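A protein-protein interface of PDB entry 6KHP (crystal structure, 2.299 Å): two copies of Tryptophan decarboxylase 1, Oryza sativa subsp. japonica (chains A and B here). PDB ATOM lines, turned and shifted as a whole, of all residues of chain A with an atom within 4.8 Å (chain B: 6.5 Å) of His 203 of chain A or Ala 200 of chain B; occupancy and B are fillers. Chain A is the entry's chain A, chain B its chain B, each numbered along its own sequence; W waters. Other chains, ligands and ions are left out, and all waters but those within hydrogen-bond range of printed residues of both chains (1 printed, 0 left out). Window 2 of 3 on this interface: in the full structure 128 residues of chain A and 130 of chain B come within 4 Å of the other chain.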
ATOM      1  N   ALA A 200     -15.723  -6.532  15.800  1.00  0.00           N
ATOM      2  CA  ALA A 200     -15.148  -5.371  15.121  1.00  0.00           C
ATOM      3  C   ALA A 200     -15.661  -4.067  15.720  1.00  0.00           C
ATOM      4  O   ALA A 200     -14.959  -3.051  15.683  1.00  0.00           O
ATOM      5  CB  ALA A 200     -15.443  -5.423  13.618  1.00  0.00           C
ATOM      6  N   GLY A 201     -16.862  -4.080  16.295  1.00  0.00           N
ATOM      7  CA  GLY A 201     -17.460  -2.892  16.858  1.00  0.00           C
ATOM      8  C   GLY A 201     -17.153  -2.642  18.310  1.00  0.00           C
ATOM      9  O   GLY A 201     -17.692  -1.690  18.882  1.00  0.00           O
ATOM     10  N   LEU A 202     -16.307  -3.470  18.934  1.00  0.00           N
ATOM     11  CA  LEU A 202     -16.022  -3.289  20.356  1.00  0.00           C
ATOM     12  C   LEU A 202     -15.372  -1.933  20.629  1.00  0.00           C
ATOM     13  O   LEU A 202     -15.644  -1.309  21.664  1.00  0.00           O
ATOM     14  CB  LEU A 202     -15.141  -4.435  20.866  1.00  0.00           C
ATOM     15  CG  LEU A 202     -14.980  -4.610  22.386  1.00  0.00           C
ATOM     16  CD1 LEU A 202     -16.262  -4.334  23.164  1.00  0.00           C
ATOM     17  CD2 LEU A 202     -14.453  -6.005  22.737  1.00  0.00           C
ATOM     18  N   HIS A 203     -14.548  -1.438  19.702  1.00  0.00           N
ATOM     19  CA  HIS A 203     -13.928  -0.132  19.891  1.00  0.00           C
ATOM     20  C   HIS A 203     -14.938   1.007  19.863  1.00  0.00           C
ATOM     21  O   HIS A 203     -14.578   2.132  20.212  1.00  0.00           O
ATOM     22  CB  HIS A 203     -12.845   0.107  18.830  1.00  0.00           C
ATOM     23  CG  HIS A 203     -13.386   0.321  17.457  1.00  0.00           C
ATOM     24  ND1 HIS A 203     -14.007   1.493  17.075  1.00  0.00           N
ATOM     25  CD2 HIS A 203     -13.416  -0.491  16.374  1.00  0.00           C
ATOM     26  CE1 HIS A 203     -14.397   1.392  15.816  1.00  0.00           C
ATOM     27  NE2 HIS A 203     -14.046   0.201  15.366  1.00  0.00           N
ATOM     28  N   ARG A 204     -16.187   0.747  19.479  1.00  0.00           N
ATOM     29  CA  ARG A 204     -17.213   1.780  19.502  1.00  0.00           C
ATOM     30  C   ARG A 204     -17.928   1.901  20.843  1.00  0.00           C
ATOM     31  O   ARG A 204     -18.659   2.878  21.043  1.00  0.00           O
ATOM     32  CB  ARG A 204     -18.249   1.516  18.405  1.00  0.00           C
ATOM     33  CG  ARG A 204     -17.867   2.049  17.029  1.00  0.00           C
ATOM     34  CD  ARG A 204     -19.092   2.674  16.319  1.00  0.00           C
ATOM     35  NE  ARG A 204     -20.248   1.769  16.290  1.00  0.00           N
ATOM     36  CZ  ARG A 204     -21.521   2.143  16.126  1.00  0.00           C
ATOM     37  NH1 ARG A 204     -21.842   3.428  15.971  1.00  0.00           N
ATOM     38  NH2 ARG A 204     -22.484   1.222  16.115  1.00  0.00           N
ATOM     39  N   LEU A 205     -17.755   0.950  21.766  1.00  0.00           N
ATOM     40  CA  LEU A 205     -18.524   0.962  23.008  1.00  0.00           C
ATOM     41  C   LEU A 205     -17.865   1.847  24.055  1.00  0.00           C
ATOM     42  O   LEU A 205     -16.636   1.916  24.145  1.00  0.00           O
ATOM     43  CB  LEU A 205     -18.676  -0.449  23.564  1.00  0.00           C
ATOM     44  CG  LEU A 205     -19.217  -1.527  22.632  1.00  0.00           C
ATOM     45  CD1 LEU A 205     -19.620  -2.737  23.452  1.00  0.00           C
ATOM     46  CD2 LEU A 205     -20.387  -1.016  21.799  1.00  0.00           C
ATOM     47  N   ASP A 227     -12.218  -0.480  25.092  1.00  0.00           N
ATOM     48  CA  ASP A 227     -11.074   0.313  24.656  1.00  0.00           C
ATOM     49  C   ASP A 227     -10.709   1.330  25.729  1.00  0.00           C
ATOM     50  O   ASP A 227     -11.591   2.042  26.215  1.00  0.00           O
ATOM     51  CB  ASP A 227     -11.373   1.041  23.348  1.00  0.00           C
ATOM     52  CG  ASP A 227     -10.114   1.580  22.681  1.00  0.00           C
ATOM     53  OD1 ASP A 227      -9.462   2.487  23.250  1.00  0.00           O
ATOM     54  OD2 ASP A 227      -9.762   1.070  21.595  1.00  0.00           O
ATOM     55  N   ASN A 230     -12.176   4.723  25.561  1.00  0.00           N
ATOM     56  CA  ASN A 230     -13.617   4.858  25.724  1.00  0.00           C
ATOM     57  C   ASN A 230     -14.079   4.619  27.150  1.00  0.00           C
ATOM     58  O   ASN A 230     -15.286   4.582  27.397  1.00  0.00           O
ATOM     59  CB  ASN A 230     -14.333   3.912  24.764  1.00  0.00           C
ATOM     60  CG  ASN A 230     -14.062   4.264  23.329  1.00  0.00           C
ATOM     61  OD1 ASN A 230     -13.854   5.427  23.017  1.00  0.00           O
ATOM     62  ND2 ASN A 230     -14.047   3.265  22.449  1.00  0.00           N
ATOM     63  N   LEU A 261     -20.441   6.768  19.119  1.00  0.00           N
ATOM     64  CA  LEU A 261     -20.094   5.710  20.053  1.00  0.00           C
ATOM     65  C   LEU A 261     -21.361   5.150  20.697  1.00  0.00           C
ATOM     66  O   LEU A 261     -22.433   5.756  20.636  1.00  0.00           O
ATOM     67  CB  LEU A 261     -19.137   6.240  21.122  1.00  0.00           C
ATOM     68  CG  LEU A 261     -17.780   6.719  20.593  1.00  0.00           C
ATOM     69  CD1 LEU A 261     -16.974   7.394  21.694  1.00  0.00           C
ATOM     70  CD2 LEU A 261     -16.996   5.567  20.003  1.00  0.00           C
ATOM     71  N   LEU B 191      -2.218  -7.353  20.307  1.00  0.00           N
ATOM     72  CA  LEU B 191      -2.747  -6.103  19.781  1.00  0.00           C
ATOM     73  C   LEU B 191      -1.616  -5.108  19.539  1.00  0.00           C
ATOM     74  O   LEU B 191      -1.622  -4.384  18.537  1.00  0.00           O
ATOM     75  CB  LEU B 191      -3.803  -5.516  20.724  1.00  0.00           C
ATOM     76  CG  LEU B 191      -5.233  -6.083  20.773  1.00  0.00           C
ATOM     77  CD1 LEU B 191      -6.030  -5.384  21.845  1.00  0.00           C
ATOM     78  CD2 LEU B 191      -5.961  -5.969  19.439  1.00  0.00           C
ATOM     79  N   SER B 196      -2.429  -2.510  16.470  1.00  0.00           N
ATOM     80  CA  SER B 196      -3.811  -2.142  16.723  1.00  0.00           C
ATOM     81  C   SER B 196      -3.882  -0.817  17.466  1.00  0.00           C
ATOM     82  O   SER B 196      -3.152  -0.592  18.437  1.00  0.00           O
ATOM     83  CB  SER B 196      -4.512  -3.232  17.535  1.00  0.00           C
ATOM     84  OG  SER B 196      -5.819  -2.828  17.914  1.00  0.00           O
ATOM     85  N   ASP B 197      -4.775   0.059  17.018  1.00  0.00           N
ATOM     86  CA  ASP B 197      -5.104   1.242  17.804  1.00  0.00           C
ATOM     87  C   ASP B 197      -6.121   0.819  18.855  1.00  0.00           C
ATOM     88  O   ASP B 197      -7.320   0.701  18.570  1.00  0.00           O
ATOM     89  CB  ASP B 197      -5.651   2.365  16.932  1.00  0.00           C
ATOM     90  CG  ASP B 197      -6.017   3.592  17.752  1.00  0.00           C
ATOM     91  OD1 ASP B 197      -5.435   3.747  18.848  1.00  0.00           O
ATOM     92  OD2 ASP B 197      -6.882   4.385  17.322  1.00  0.00           O
ATOM     93  N   GLY B 198      -5.644   0.601  20.075  1.00  0.00           N
ATOM     94  CA  GLY B 198      -6.520   0.091  21.115  1.00  0.00           C
ATOM     95  C   GLY B 198      -7.068  -1.254  20.694  1.00  0.00           C
ATOM     96  O   GLY B 198      -6.334  -2.121  20.213  1.00  0.00           O
ATOM     97  N   VAL B 199      -8.383  -1.421  20.822  1.00  0.00           N
ATOM     98  CA  VAL B 199      -8.977  -2.727  20.568  1.00  0.00           C
ATOM     99  C   VAL B 199      -9.508  -2.785  19.142  1.00  0.00           C
ATOM    100  O   VAL B 199     -10.158  -3.761  18.753  1.00  0.00           O
ATOM    101  CB  VAL B 199     -10.074  -3.066  21.599  1.00  0.00           C
ATOM    102  CG1 VAL B 199      -9.501  -3.021  23.022  1.00  0.00           C
ATOM    103  CG2 VAL B 199     -11.271  -2.129  21.473  1.00  0.00           C
ATOM    104  N   ALA B 200      -9.187  -1.767  18.337  1.00  0.00           N
ATOM    105  CA  ALA B 200      -9.729  -1.689  16.984  1.00  0.00           C
ATOM    106  C   ALA B 200      -9.374  -2.916  16.146  1.00  0.00           C
ATOM    107  O   ALA B 200     -10.185  -3.358  15.323  1.00  0.00           O
ATOM    108  CB  ALA B 200      -9.254  -0.399  16.299  1.00  0.00           C
ATOM    109  N   GLY B 201      -8.193  -3.496  16.345  1.00  0.00           N
ATOM    110  CA  GLY B 201      -7.816  -4.708  15.639  1.00  0.00           C
ATOM    111  C   GLY B 201      -8.158  -6.013  16.332  1.00  0.00           C
ATOM    112  O   GLY B 201      -7.690  -7.078  15.910  1.00  0.00           O
ATOM    113  N   LEU B 202      -8.978  -5.963  17.383  1.00  0.00           N
ATOM    114  CA  LEU B 202      -9.311  -7.164  18.139  1.00  0.00           C
ATOM    115  C   LEU B 202      -9.969  -8.227  17.267  1.00  0.00           C
ATOM    116  O   LEU B 202      -9.736  -9.425  17.467  1.00  0.00           O
ATOM    117  CB  LEU B 202     -10.214  -6.777  19.302  1.00  0.00           C
ATOM    118  CG  LEU B 202     -10.589  -7.826  20.334  1.00  0.00           C
ATOM    119  CD1 LEU B 202      -9.346  -8.571  20.834  1.00  0.00           C
ATOM    120  CD2 LEU B 202     -11.313  -7.101  21.453  1.00  0.00           C
ATOM    121  N   HIS B 203     -10.765  -7.816  16.280  1.00  0.00           N
ATOM    122  CA  HIS B 203     -11.428  -8.754  15.377  1.00  0.00           C
ATOM    123  C   HIS B 203     -10.460  -9.510  14.475  1.00  0.00           C
ATOM    124  O   HIS B 203     -10.897 -10.426  13.772  1.00  0.00           O
ATOM    125  CB  HIS B 203     -12.450  -8.017  14.510  1.00  0.00           C
ATOM    126  CG  HIS B 203     -11.824  -7.120  13.488  1.00  0.00           C
ATOM    127  ND1 HIS B 203     -11.293  -5.886  13.807  1.00  0.00           N
ATOM    128  CD2 HIS B 203     -11.608  -7.291  12.162  1.00  0.00           C
ATOM    129  CE1 HIS B 203     -10.797  -5.328  12.717  1.00  0.00           C
ATOM    130  NE2 HIS B 203     -10.974  -6.161  11.705  1.00  0.00           N
ATOM    131  N   ARG B 204      -9.176  -9.164  14.469  1.00  0.00           N
ATOM    132  CA  ARG B 204      -8.198  -9.935  13.706  1.00  0.00           C
ATOM    133  C   ARG B 204      -7.513 -11.033  14.515  1.00  0.00           C
ATOM    134  O   ARG B 204      -6.790 -11.842  13.924  1.00  0.00           O
ATOM    135  CB  ARG B 204      -7.120  -9.007  13.140  1.00  0.00           C
ATOM    136  CG  ARG B 204      -7.672  -7.685  12.616  1.00  0.00           C
ATOM    137  CD  ARG B 204      -6.615  -6.873  11.893  1.00  0.00           C
ATOM    138  NE  ARG B 204      -5.717  -7.711  11.105  1.00  0.00           N
ATOM    139  CZ  ARG B 204      -4.393  -7.631  11.172  1.00  0.00           C
ATOM    140  NH1 ARG B 204      -3.834  -6.737  11.989  1.00  0.00           N
ATOM    141  NH2 ARG B 204      -3.627  -8.421  10.419  1.00  0.00           N
HETATM  142  O   HOH W   1      -9.501   2.670  19.507  1.00  0.00           O
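The side-chain carboxylate (OD2) of Asp 227 of chain A lies within hydrogen-bond range of the backbone NH (N) of Val 199 of chain B.
The backbone carbonyl oxygen of Ala 200 of chain A sits close to a ring nitrogen (NE2) of His 203 of chain A, 3.4 Å away.
The backbone carbonyl oxygen (O) of His 203 of chain A lies within hydrogen-bond range of the side-chain amide nitrogen (ND2) of Asn 230 of chain A (2.6 Å).
OG of Ser 196 of chain B sits at hydrogen-bond distance from O of Gly 198 of chain B.
A ring nitrogen (ND1) of His 203 of chain B is in hydrogen-bond range of the backbone carbonyl oxygen (O) of Ala 200 of chain B (3.1 Å).
Ala 200 of chain A touches His 203 of chain B.
Leu 202 of chain B touches Leu 202 of chain A.
CA of His 203 of chain A touches CG2 of Val 199 of chain B (3.7 Å).
CD2 of His 203 of chain A touches CA of Ala 200 of chain B, at 3.9 Å.
OD2 of Asp 227 of chain A touches O of Asp 197 of chain B, 3.9 Å away.
Gly 198 of chain B touches Asp 227 of chain A.
His 203 of chain A touches just these residues of chain B: Val 199 and Ala 200.
Printed residues of chain B within 4 Å of Asp 227 of chain A: Asp 197, Gly 198 and Val 199.
Asn 230 of chain A touches none of the printed residues of chain B.
Ser 196 of chain B touches none of the printed residues of chain A.
Of the printed residues of chain A, Gly 198 of chain B touches Asp 227.
Of the printed residues of chain A, Val 199 of chain B touches His 203 (3.7 Å) and Asp 227 (3.0 Å).
Of chain A, only His 203 comes within 4 Å of Ala 200 of chain B.
Of the printed residues of chain A, Leu 202 of chain B touches Leu 202 (3.6 Å).
Of the printed residues of chain A, His 203 of chain B touches Ala 200 (3.8 Å).
The nearest residue of chain A that does not touch Ala 200 of chain B is Asp 227 of chain A (4.4 Å).
The nearest printed residue of chain A that does not touch Gly 198 of chain B is His 203 of chain A (6.2 Å).
Printed residues of chain A that touch a printed residue of chain B: Ala 200, Leu 202, His 203 and Asp 227.
Of the 10 printed residues of chain B, 6 touch a printed residue of chain A.
Printed residues of chain B that touch a printed residue of chain A: Asp 197, Gly 198, Val 199, Ala 200, Leu 202 and His 203.
Among the printed residues, 7 pairs touch across the chains.
Among the printed residues, no Asp or Glu carboxylate lies within 4 Å of a Lys or Arg side-chain nitrogen of the other chain.
Ala 200 of chain A touches His 203 of chain B, and with the chains exchanged His 203 of chain A touches Ala 200 of chain B.
Leu 202 of chain A touches its own counterpart, Leu 202 of chain B.
Of the 7 pairs that touch across the chains among the printed residues, 3 have their exchanged pair printed and touching as well.
Water W1 lies within hydrogen-bond range of OD2 of Asp 227 of chain A (2.6 Å) and O of Asp 197 of chain B (3.1 Å).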
